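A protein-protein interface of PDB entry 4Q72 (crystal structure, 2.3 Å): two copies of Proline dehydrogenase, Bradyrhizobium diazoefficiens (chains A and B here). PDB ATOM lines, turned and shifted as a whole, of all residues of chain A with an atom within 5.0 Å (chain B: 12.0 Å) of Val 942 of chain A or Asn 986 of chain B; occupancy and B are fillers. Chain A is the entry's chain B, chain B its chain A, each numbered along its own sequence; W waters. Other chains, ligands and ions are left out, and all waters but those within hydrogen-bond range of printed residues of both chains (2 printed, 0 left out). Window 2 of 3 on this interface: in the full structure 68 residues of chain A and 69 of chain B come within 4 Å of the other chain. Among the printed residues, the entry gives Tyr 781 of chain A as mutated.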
ATOM      1  N   LYS A 353     -29.030   5.326   5.172  1.00  0.00           N
ATOM      2  CA  LYS A 353     -27.921   5.796   4.351  1.00  0.00           C
ATOM      3  C   LYS A 353     -28.410   6.818   3.331  1.00  0.00           C
ATOM      4  O   LYS A 353     -27.797   7.881   3.164  1.00  0.00           O
ATOM      5  CB  LYS A 353     -27.239   4.616   3.653  1.00  0.00           C
ATOM      6  CG  LYS A 353     -26.020   4.986   2.820  1.00  0.00           C
ATOM      7  CD  LYS A 353     -25.318   3.748   2.281  1.00  0.00           C
ATOM      8  CE  LYS A 353     -24.098   4.104   1.449  1.00  0.00           C
ATOM      9  NZ  LYS A 353     -23.274   2.905   1.057  1.00  0.00           N
ATOM     10  N   TYR A 781     -23.885   1.340 -11.274  1.00  0.00           N
ATOM     11  CA  TYR A 781     -22.730   2.181 -10.986  1.00  0.00           C
ATOM     12  C   TYR A 781     -22.014   2.617 -12.271  1.00  0.00           C
ATOM     13  O   TYR A 781     -21.475   3.728 -12.345  1.00  0.00           O
ATOM     14  CB  TYR A 781     -21.763   1.450 -10.051  1.00  0.00           C
ATOM     15  CG  TYR A 781     -22.372   1.104  -8.700  1.00  0.00           C
ATOM     16  CD1 TYR A 781     -23.308   1.942  -8.097  1.00  0.00           C
ATOM     17  CD2 TYR A 781     -22.029  -0.078  -8.038  1.00  0.00           C
ATOM     18  CE1 TYR A 781     -23.868   1.627  -6.867  1.00  0.00           C
ATOM     19  CE2 TYR A 781     -22.593  -0.409  -6.803  1.00  0.00           C
ATOM     20  CZ  TYR A 781     -23.513   0.442  -6.227  1.00  0.00           C
ATOM     21  OH  TYR A 781     -24.062   0.124  -5.010  1.00  0.00           O
ATOM     22  N   VAL A 920     -13.597   0.014  -8.200  1.00  0.00           N
ATOM     23  CA  VAL A 920     -13.271  -1.387  -7.984  1.00  0.00           C
ATOM     24  C   VAL A 920     -14.511  -2.129  -7.504  1.00  0.00           C
ATOM     25  O   VAL A 920     -15.144  -1.753  -6.505  1.00  0.00           O
ATOM     26  CB  VAL A 920     -12.155  -1.575  -6.922  1.00  0.00           C
ATOM     27  CG1 VAL A 920     -11.779  -3.061  -6.797  1.00  0.00           C
ATOM     28  CG2 VAL A 920     -10.930  -0.740  -7.268  1.00  0.00           C
ATOM     29  N   ILE A 928      -9.310  -6.259  -3.743  1.00  0.00           N
ATOM     30  CA  ILE A 928      -9.524  -4.833  -3.522  1.00  0.00           C
ATOM     31  C   ILE A 928      -8.277  -4.178  -2.942  1.00  0.00           C
ATOM     32  O   ILE A 928      -7.787  -3.169  -3.466  1.00  0.00           O
ATOM     33  CB  ILE A 928     -10.707  -4.614  -2.570  1.00  0.00           C
ATOM     34  CG1 ILE A 928     -11.965  -5.225  -3.193  1.00  0.00           C
ATOM     35  CG2 ILE A 928     -10.902  -3.112  -2.254  1.00  0.00           C
ATOM     36  CD1 ILE A 928     -13.136  -5.267  -2.262  1.00  0.00           C
ATOM     37  N   ILE A 932      -5.742  -1.369  -4.511  1.00  0.00           N
ATOM     38  CA  ILE A 932      -5.469  -0.125  -3.792  1.00  0.00           C
ATOM     39  C   ILE A 932      -3.966   0.071  -3.563  1.00  0.00           C
ATOM     40  O   ILE A 932      -3.431   1.145  -3.831  1.00  0.00           O
ATOM     41  CB  ILE A 932      -6.226  -0.081  -2.462  1.00  0.00           C
ATOM     42  CG1 ILE A 932      -7.727   0.049  -2.733  1.00  0.00           C
ATOM     43  CG2 ILE A 932      -5.717   1.073  -1.572  1.00  0.00           C
ATOM     44  CD1 ILE A 932      -8.621  -0.265  -1.499  1.00  0.00           C
ATOM     45  N   ILE A 940     -10.322   6.455  -4.925  1.00  0.00           N
ATOM     46  CA  ILE A 940     -10.699   5.078  -5.214  1.00  0.00           C
ATOM     47  C   ILE A 940     -12.085   4.834  -4.634  1.00  0.00           C
ATOM     48  O   ILE A 940     -12.353   5.174  -3.474  1.00  0.00           O
ATOM     49  CB  ILE A 940      -9.659   4.083  -4.649  1.00  0.00           C
ATOM     50  CG1 ILE A 940      -8.295   4.343  -5.286  1.00  0.00           C
ATOM     51  CG2 ILE A 940     -10.102   2.623  -4.870  1.00  0.00           C
ATOM     52  CD1 ILE A 940      -7.171   3.583  -4.646  1.00  0.00           C
ATOM     53  N   TYR A 941     -12.975   4.307  -5.469  1.00  0.00           N
ATOM     54  CA  TYR A 941     -14.353   4.015  -5.075  1.00  0.00           C
ATOM     55  C   TYR A 941     -14.667   2.526  -5.216  1.00  0.00           C
ATOM     56  O   TYR A 941     -14.607   1.958  -6.319  1.00  0.00           O
ATOM     57  CB  TYR A 941     -15.335   4.819  -5.924  1.00  0.00           C
ATOM     58  CG  TYR A 941     -15.299   6.314  -5.689  1.00  0.00           C
ATOM     59  CD1 TYR A 941     -14.571   7.156  -6.526  1.00  0.00           C
ATOM     60  CD2 TYR A 941     -16.010   6.887  -4.643  1.00  0.00           C
ATOM     61  CE1 TYR A 941     -14.547   8.524  -6.328  1.00  0.00           C
ATOM     62  CE2 TYR A 941     -15.982   8.258  -4.423  1.00  0.00           C
ATOM     63  CZ  TYR A 941     -15.253   9.074  -5.275  1.00  0.00           C
ATOM     64  OH  TYR A 941     -15.229  10.444  -5.072  1.00  0.00           O
ATOM     65  N   VAL A 942     -15.017   1.906  -4.099  1.00  0.00           N
ATOM     66  CA  VAL A 942     -15.196   0.472  -4.040  1.00  0.00           C
ATOM     67  C   VAL A 942     -16.668   0.096  -3.888  1.00  0.00           C
ATOM     68  O   VAL A 942     -17.328   0.500  -2.927  1.00  0.00           O
ATOM     69  CB  VAL A 942     -14.380  -0.140  -2.878  1.00  0.00           C
ATOM     70  CG1 VAL A 942     -14.573  -1.660  -2.831  1.00  0.00           C
ATOM     71  CG2 VAL A 942     -12.921   0.184  -3.044  1.00  0.00           C
ATOM     72  N   ASN A 943     -17.171  -0.677  -4.846  1.00  0.00           N
ATOM     73  CA  ASN A 943     -18.562  -1.147  -4.842  1.00  0.00           C
ATOM     74  C   ASN A 943     -19.611  -0.020  -4.742  1.00  0.00           C
ATOM     75  O   ASN A 943     -20.634  -0.170  -4.087  1.00  0.00           O
ATOM     76  CB  ASN A 943     -18.766  -2.243  -3.772  1.00  0.00           C
ATOM     77  CG  ASN A 943     -17.982  -3.513  -4.093  1.00  0.00           C
ATOM     78  OD1 ASN A 943     -17.882  -3.907  -5.267  1.00  0.00           O
ATOM     79  ND2 ASN A 943     -17.391  -4.136  -3.072  1.00  0.00           N
ATOM     80  N   ARG A 944     -19.338   1.108  -5.395  1.00  0.00           N
ATOM     81  CA  ARG A 944     -20.317   2.183  -5.525  1.00  0.00           C
ATOM     82  C   ARG A 944     -19.913   2.965  -6.763  1.00  0.00           C
ATOM     83  O   ARG A 944     -18.916   2.620  -7.415  1.00  0.00           O
ATOM     84  CB  ARG A 944     -20.343   3.084  -4.268  1.00  0.00           C
ATOM     85  CG  ARG A 944     -18.981   3.588  -3.803  1.00  0.00           C
ATOM     86  CD  ARG A 944     -19.090   4.939  -3.086  1.00  0.00           C
ATOM     87  NE  ARG A 944     -19.304   6.015  -4.044  1.00  0.00           N
ATOM     88  CZ  ARG A 944     -19.537   7.282  -3.722  1.00  0.00           C
ATOM     89  NH1 ARG A 944     -19.701   8.185  -4.687  1.00  0.00           N
ATOM     90  NH2 ARG A 944     -19.589   7.644  -2.442  1.00  0.00           N
ATOM     91  N   GLU B 632      -4.093   6.189   8.546  1.00  0.00           N
ATOM     92  CA  GLU B 632      -5.048   6.912   7.724  1.00  0.00           C
ATOM     93  C   GLU B 632      -5.914   7.819   8.592  1.00  0.00           C
ATOM     94  O   GLU B 632      -6.037   7.610   9.802  1.00  0.00           O
ATOM     95  CB  GLU B 632      -5.938   5.916   6.991  1.00  0.00           C
ATOM     96  CG  GLU B 632      -6.738   5.006   7.920  1.00  0.00           C
ATOM     97  CD  GLU B 632      -7.444   3.882   7.167  1.00  0.00           C
ATOM     98  OE1 GLU B 632      -6.897   3.423   6.134  1.00  0.00           O
ATOM     99  OE2 GLU B 632      -8.543   3.460   7.602  1.00  0.00           O
ATOM    100  N   MET B 635     -12.576   9.929   7.611  1.00  0.00           N
ATOM    101  CA  MET B 635     -13.407  11.090   7.329  1.00  0.00           C
ATOM    102  C   MET B 635     -14.828  10.775   7.753  1.00  0.00           C
ATOM    103  O   MET B 635     -15.270   9.650   7.614  1.00  0.00           O
ATOM    104  CB  MET B 635     -13.390  11.461   5.835  1.00  0.00           C
ATOM    105  CG  MET B 635     -12.012  11.479   5.196  1.00  0.00           C
ATOM    106  SD  MET B 635     -10.875  12.692   5.883  1.00  0.00           S
ATOM    107  CE  MET B 635     -11.678  14.220   5.379  1.00  0.00           C
ATOM    108  N   GLY B 637     -18.874  10.661   7.477  1.00  0.00           N
ATOM    109  CA  GLY B 637     -19.658  10.383   6.304  1.00  0.00           C
ATOM    110  C   GLY B 637     -20.923   9.643   6.628  1.00  0.00           C
ATOM    111  O   GLY B 637     -21.284   9.481   7.783  1.00  0.00           O
ATOM    112  N   PRO B 638     -21.609   9.175   5.593  1.00  0.00           N
ATOM    113  CA  PRO B 638     -22.868   8.489   5.860  1.00  0.00           C
ATOM    114  C   PRO B 638     -22.584   7.122   6.442  1.00  0.00           C
ATOM    115  O   PRO B 638     -21.441   6.672   6.370  1.00  0.00           O
ATOM    116  CB  PRO B 638     -23.501   8.384   4.471  1.00  0.00           C
ATOM    117  CG  PRO B 638     -22.327   8.364   3.525  1.00  0.00           C
ATOM    118  CD  PRO B 638     -21.257   9.207   4.161  1.00  0.00           C
ATOM    119  N   THR B 639     -23.589   6.514   7.065  1.00  0.00           N
ATOM    120  CA  THR B 639     -23.531   5.130   7.513  1.00  0.00           C
ATOM    121  C   THR B 639     -23.456   4.216   6.263  1.00  0.00           C
ATOM    122  O   THR B 639     -23.815   4.637   5.162  1.00  0.00           O
ATOM    123  CB  THR B 639     -24.804   4.791   8.342  1.00  0.00           C
ATOM    124  OG1 THR B 639     -24.722   3.459   8.873  1.00  0.00           O
ATOM    125  CG2 THR B 639     -26.074   4.908   7.472  1.00  0.00           C
ATOM    126  N   GLY B 640     -22.999   2.974   6.428  1.00  0.00           N
ATOM    127  CA  GLY B 640     -22.849   2.059   5.306  1.00  0.00           C
ATOM    128  C   GLY B 640     -21.725   2.428   4.334  1.00  0.00           C
ATOM    129  O   GLY B 640     -21.716   1.965   3.187  1.00  0.00           O
ATOM    130  N   GLU B 641     -20.780   3.262   4.778  1.00  0.00           N
ATOM    131  CA  GLU B 641     -19.689   3.685   3.905  1.00  0.00           C
ATOM    132  C   GLU B 641     -18.484   4.120   4.719  1.00  0.00           C
ATOM    133  O   GLU B 641     -18.625   4.818   5.715  1.00  0.00           O
ATOM    134  CB  GLU B 641     -20.154   4.831   2.988  1.00  0.00           C
ATOM    135  CG  GLU B 641     -19.212   5.175   1.851  1.00  0.00           C
ATOM    136  CD  GLU B 641     -19.649   6.430   1.095  1.00  0.00           C
ATOM    137  OE1 GLU B 641     -19.394   7.567   1.591  1.00  0.00           O
ATOM    138  OE2 GLU B 641     -20.264   6.272   0.013  1.00  0.00           O
ATOM    139  N   SER B 642     -17.293   3.707   4.299  1.00  0.00           N
ATOM    140  CA  SER B 642     -16.074   4.188   4.932  1.00  0.00           C
ATOM    141  C   SER B 642     -15.298   5.075   3.965  1.00  0.00           C
ATOM    142  O   SER B 642     -15.314   4.858   2.737  1.00  0.00           O
ATOM    143  CB  SER B 642     -15.196   3.036   5.440  1.00  0.00           C
ATOM    144  OG  SER B 642     -14.551   2.341   4.378  1.00  0.00           O
ATOM    145  N   ASN B 643     -14.655   6.079   4.539  1.00  0.00           N
ATOM    146  CA  ASN B 643     -13.855   7.065   3.827  1.00  0.00           C
ATOM    147  C   ASN B 643     -12.585   7.307   4.608  1.00  0.00           C
ATOM    148  O   ASN B 643     -12.633   7.739   5.762  1.00  0.00           O
ATOM    149  CB  ASN B 643     -14.616   8.386   3.640  1.00  0.00           C
ATOM    150  CG  ASN B 643     -15.781   8.251   2.676  1.00  0.00           C
ATOM    151  OD1 ASN B 643     -15.600   8.358   1.464  1.00  0.00           O
ATOM    152  ND2 ASN B 643     -16.979   8.011   3.206  1.00  0.00           N
ATOM    153  N   ALA B 644     -11.458   6.978   3.986  1.00  0.00           N
ATOM    154  CA  ALA B 644     -10.158   7.055   4.628  1.00  0.00           C
ATOM    155  C   ALA B 644      -9.178   7.819   3.761  1.00  0.00           C
ATOM    156  O   ALA B 644      -9.054   7.554   2.563  1.00  0.00           O
ATOM    157  CB  ALA B 644      -9.619   5.655   4.927  1.00  0.00           C
ATOM    158  N   THR B 646      -5.223   8.918   3.092  1.00  0.00           N
ATOM    159  CA  THR B 646      -3.853   8.497   3.321  1.00  0.00           C
ATOM    160  C   THR B 646      -2.894   9.410   2.555  1.00  0.00           C
ATOM    161  O   THR B 646      -3.313  10.174   1.688  1.00  0.00           O
ATOM    162  CB  THR B 646      -3.636   7.040   2.871  1.00  0.00           C
ATOM    163  OG1 THR B 646      -4.282   6.842   1.613  1.00  0.00           O
ATOM    164  CG2 THR B 646      -4.237   6.073   3.873  1.00  0.00           C
ATOM    165  N   ARG B 648       0.800   9.137   0.469  1.00  0.00           N
ATOM    166  CA  ARG B 648       1.703   8.166  -0.107  1.00  0.00           C
ATOM    167  C   ARG B 648       2.894   8.888  -0.709  1.00  0.00           C
ATOM    168  O   ARG B 648       2.800  10.069  -1.054  1.00  0.00           O
ATOM    169  CB  ARG B 648       0.964   7.358  -1.189  1.00  0.00           C
ATOM    170  CG  ARG B 648      -0.241   6.586  -0.694  1.00  0.00           C
ATOM    171  CD  ARG B 648      -0.986   5.904  -1.854  1.00  0.00           C
ATOM    172  NE  ARG B 648      -0.141   4.976  -2.608  1.00  0.00           N
ATOM    173  CZ  ARG B 648      -0.499   3.747  -2.992  1.00  0.00           C
ATOM    174  NH1 ARG B 648       0.367   3.006  -3.678  1.00  0.00           N
ATOM    175  NH2 ARG B 648      -1.709   3.252  -2.702  1.00  0.00           N
ATOM    176  N   GLN B 981      -4.425  10.176  -1.016  1.00  0.00           N
ATOM    177  CA  GLN B 981      -5.307   9.194  -1.645  1.00  0.00           C
ATOM    178  C   GLN B 981      -6.499   8.940  -0.733  1.00  0.00           C
ATOM    179  O   GLN B 981      -6.340   8.724   0.470  1.00  0.00           O
ATOM    180  CB  GLN B 981      -4.553   7.905  -1.965  1.00  0.00           C
ATOM    181  CG  GLN B 981      -5.438   6.753  -2.393  1.00  0.00           C
ATOM    182  CD  GLN B 981      -4.634   5.559  -2.866  1.00  0.00           C
ATOM    183  OE1 GLN B 981      -4.228   4.712  -2.068  1.00  0.00           O
ATOM    184  NE2 GLN B 981      -4.393   5.491  -4.174  1.00  0.00           N
ATOM    185  N   THR B 982      -7.690   9.045  -1.306  1.00  0.00           N
ATOM    186  CA  THR B 982      -8.923   8.773  -0.590  1.00  0.00           C
ATOM    187  C   THR B 982      -9.483   7.426  -1.071  1.00  0.00           C
ATOM    188  O   THR B 982      -9.655   7.199  -2.272  1.00  0.00           O
ATOM    189  CB  THR B 982      -9.941   9.905  -0.827  1.00  0.00           C
ATOM    190  OG1 THR B 982      -9.353  11.151  -0.436  1.00  0.00           O
ATOM    191  CG2 THR B 982     -11.226   9.683  -0.024  1.00  0.00           C
ATOM    192  N   VAL B 983      -9.740   6.529  -0.128  1.00  0.00           N
ATOM    193  CA  VAL B 983     -10.385   5.262  -0.433  1.00  0.00           C
ATOM    194  C   VAL B 983     -11.786   5.267   0.145  1.00  0.00           C
ATOM    195  O   VAL B 983     -11.973   5.452   1.356  1.00  0.00           O
ATOM    196  CB  VAL B 983      -9.627   4.067   0.144  1.00  0.00           C
ATOM    197  CG1 VAL B 983     -10.474   2.774  -0.051  1.00  0.00           C
ATOM    198  CG2 VAL B 983      -8.258   3.948  -0.501  1.00  0.00           C
ATOM    199  N   THR B 984     -12.767   5.086  -0.723  1.00  0.00           N
ATOM    200  CA  THR B 984     -14.151   5.125  -0.316  1.00  0.00           C
ATOM    201  C   THR B 984     -14.786   3.763  -0.591  1.00  0.00           C
ATOM    202  O   THR B 984     -14.851   3.319  -1.732  1.00  0.00           O
ATOM    203  CB  THR B 984     -14.927   6.231  -1.059  1.00  0.00           C
ATOM    204  OG1 THR B 984     -14.379   7.516  -0.721  1.00  0.00           O
ATOM    205  CG2 THR B 984     -16.395   6.189  -0.690  1.00  0.00           C
ATOM    206  N   ILE B 985     -15.246   3.114   0.473  1.00  0.00           N
ATOM    207  CA  ILE B 985     -15.803   1.779   0.373  1.00  0.00           C
ATOM    208  C   ILE B 985     -17.255   1.702   0.826  1.00  0.00           C
ATOM    209  O   ILE B 985     -17.586   2.056   1.951  1.00  0.00           O
ATOM    210  CB  ILE B 985     -15.014   0.774   1.220  1.00  0.00           C
ATOM    211  CG1 ILE B 985     -13.534   0.820   0.859  1.00  0.00           C
ATOM    212  CG2 ILE B 985     -15.633  -0.654   1.063  1.00  0.00           C
ATOM    213  CD1 ILE B 985     -12.650   0.017   1.787  1.00  0.00           C
ATOM    214  N   ASN B 986     -18.102   1.188  -0.057  1.00  0.00           N
ATOM    215  CA  ASN B 986     -19.491   0.924   0.264  1.00  0.00           C
ATOM    216  C   ASN B 986     -19.540  -0.326   1.146  1.00  0.00           C
ATOM    217  O   ASN B 986     -19.293  -1.436   0.698  1.00  0.00           O
ATOM    218  CB  ASN B 986     -20.287   0.787  -1.036  1.00  0.00           C
ATOM    219  CG  ASN B 986     -21.731   0.310  -0.829  1.00  0.00           C
ATOM    220  OD1 ASN B 986     -22.208   0.142   0.294  1.00  0.00           O
ATOM    221  ND2 ASN B 986     -22.429   0.098  -1.939  1.00  0.00           N
ATOM    222  N   THR B 987     -19.846  -0.132   2.416  1.00  0.00           N
ATOM    223  CA  THR B 987     -19.729  -1.219   3.358  1.00  0.00           C
ATOM    224  C   THR B 987     -21.080  -1.824   3.681  1.00  0.00           C
ATOM    225  O   THR B 987     -21.155  -2.726   4.502  1.00  0.00           O
ATOM    226  CB  THR B 987     -19.016  -0.766   4.669  1.00  0.00           C
ATOM    227  OG1 THR B 987     -19.786   0.243   5.329  1.00  0.00           O
ATOM    228  CG2 THR B 987     -17.631  -0.223   4.366  1.00  0.00           C
ATOM    229  N   ALA B 988     -22.132  -1.360   3.005  1.00  0.00           N
ATOM    230  CA  ALA B 988     -23.508  -1.763   3.331  1.00  0.00           C
ATOM    231  C   ALA B 988     -23.799  -3.274   3.303  1.00  0.00           C
ATOM    232  O   ALA B 988     -24.662  -3.748   4.050  1.00  0.00           O
ATOM    233  CB  ALA B 988     -24.517  -1.020   2.452  1.00  0.00           C
ATOM    234  N   ALA B 989     -23.111  -4.025   2.446  1.00  0.00           N
ATOM    235  CA  ALA B 989     -23.343  -5.475   2.381  1.00  0.00           C
ATOM    236  C   ALA B 989     -22.872  -6.233   3.636  1.00  0.00           C
ATOM    237  O   ALA B 989     -23.330  -7.357   3.900  1.00  0.00           O
ATOM    238  CB  ALA B 989     -22.729  -6.083   1.115  1.00  0.00           C
ATOM    239  N   ALA B 990     -21.973  -5.620   4.408  1.00  0.00           N
ATOM    240  CA  ALA B 990     -21.494  -6.243   5.642  1.00  0.00           C
ATOM    241  C   ALA B 990     -22.521  -6.097   6.769  1.00  0.00           C
ATOM    242  O   ALA B 990     -22.611  -6.954   7.654  1.00  0.00           O
ATOM    243  CB  ALA B 990     -20.147  -5.651   6.065  1.00  0.00           C
ATOM    244  N   GLY B 991     -23.298  -5.015   6.717  1.00  0.00           N
ATOM    245  CA  GLY B 991     -24.311  -4.728   7.721  1.00  0.00           C
ATOM    246  C   GLY B 991     -23.920  -3.622   8.684  1.00  0.00           C
ATOM    247  O   GLY B 991     -22.792  -3.588   9.169  1.00  0.00           O
HETATM  248  O   HOH W   1     -17.182  -3.226  -0.144  1.00  0.00           O
HETATM  249  O   HOH W   2     -12.769   8.332  -3.024  1.00  0.00           O
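The guanidinium group of Arg 648 of chain B is in hydrogen-bond range of the backbone carbonyl oxygen of Ile 932 of chain A.
OE2 of Glu 641 of chain B is in salt-bridge range of NH2 of Arg 944 of chain A, 2.9 Å away.
N of Thr 984 of chain B lies within hydrogen-bond range of O of Ile 940 of chain A.
The side-chain amide oxygen of Asn 986 of chain B is in hydrogen-bond range of the side-chain amino group of Lys 353 of chain A, at 3.1 Å.
The backbone carbonyl oxygen of Thr 984 of chain B sits at hydrogen-bond distance from the backbone NH of Val 942 of chain A (2.8 Å).
ND2 of Asn 986 of chain B lies within hydrogen-bond range of OH of Tyr 781 of chain A (3.5 Å).
NZ of Lys 353 of chain A is in hydrogen-bond range of O of Gly 640 of chain B (2.8 Å).
The backbone carbonyl oxygen (O) of Thr 982 of chain B is in hydrogen-bond range of the backbone NH (N) of Ile 940 of chain A.
The backbone carbonyl oxygen (O) of Val 942 of chain A is in hydrogen-bond range of the backbone NH (N) of Asn 986 of chain B, at 3.1 Å.
The side-chain amide nitrogen of Asn 986 of chain B is in hydrogen-bond range of the backbone carbonyl oxygen of Asn 943 of chain A, 2.8 Å away.
The backbone carbonyl oxygen (O) of Gly 640 of chain B lies within hydrogen-bond range of the backbone NH (N) of Thr 987 of chain B (2.9 Å).
NH2 of Arg 648 of chain B lies within hydrogen-bond range of OE1 of Gln 981 of chain B, 3.0 Å away.
The side-chain hydroxyl (OG1) of Thr 984 of chain B sits at hydrogen-bond distance from the side-chain amide oxygen (OD1) of Asn 643 of chain B (2.6 Å).
N of Thr 646 of chain B lies within hydrogen-bond range of O of Gln 981 of chain B (2.9 Å).
OE1 of Glu 641 of chain B lies within hydrogen-bond range of ND2 of Asn 643 of chain B, at 2.9 Å.
The backbone carbonyl oxygen (O) of Val 920 of chain A lies within hydrogen-bond range of the backbone NH (N) of Asn 943 of chain A (2.8 Å).
Among the printed residues, merely in contact across the chains: Lys 353 of chain A with Thr 639 of chain B, Ile 940 of chain A with Gln 981 of chain B, Tyr 941 of chain A with Thr 984 of chain B, Ile 940 of chain A with Val 983 of chain B, Arg 944 of chain A with Thr 984 of chain B, Ile 932 of chain A with Val 983 of chain B, Val 942 of chain A with Ile 985 of chain B, Ile 932 of chain A with Gln 981 of chain B and Arg 944 of chain A with Asn 986 of chain B.
Val 942 of chain A touches just these residues of chain B: Thr 984, Ile 985 and Asn 986.
Asn 986 of chain B touches just these residues of chain A: Lys 353 (3.1 Å), Tyr 781 (3.5 Å), Val 942 (3.1 Å), Asn 943 (2.8 Å) and Arg 944 (3.97 Å).
No residue of chain B comes within 4 Å of Val 920 of chain A.
Of chain B, only Gln 981, Thr 982, Val 983 and Thr 984 come within 4 Å of Ile 940 of chain A.
Arg 944 of chain A touches just these residues of chain B: Glu 641, Thr 984 and Asn 986.
Of the printed residues of chain B, Tyr 781 of chain A touches Asn 986 (3.5 Å).
Of the printed residues of chain A, Thr 982 of chain B touches Ile 940 (2.8 Å).
Of the printed residues of chain B, Ile 932 of chain A touches Arg 648 (2.9 Å), Gln 981 (3.96 Å) and Val 983 (3.8 Å).
Of the printed residues of chain A, Gly 640 of chain B touches Lys 353 (2.8 Å).
Of the printed residues of chain A, Val 983 of chain B touches Ile 932 (3.8 Å) and Ile 940 (3.6 Å).
Glu 632 of chain B touches none of the printed residues of chain A.
Asn 643 of chain B touches none of the printed residues of chain A.
The nearest residue of chain B that does not touch Val 942 of chain A is Val 983 of chain B (4.7 Å).
Of the 10 printed residues of chain A, 8 touch a printed residue of chain B.
Printed residues of chain A that touch a printed residue of chain B: Lys 353, Tyr 781, Ile 932, Ile 940, Tyr 941, Val 942, Asn 943 and Arg 944.
Hydrophobic or aromatic side chains of chain A that line the printed part of chain B: Tyr 781, Ile 932, Ile 940, Tyr 941 and Val 942.
Among the printed residues, Asp or Glu carboxylates within 4 Å of a Lys or Arg side-chain nitrogen of the other chain: Arg 944 of chain A with Glu 641 of chain B.
No position is printed for both chains.
Water W1 lies within hydrogen-bond range of the backbone carbonyl oxygen (O) of Asn 986 of chain B and the side-chain amide nitrogen (ND2) of Asn 943 of chain A.
Water W2 lies within hydrogen-bond range of OG1 of Thr 984 of chain B (2.9 Å), O of Ile 940 of chain A (3.2 Å) and O of Thr 982 of chain B (3.4 Å).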
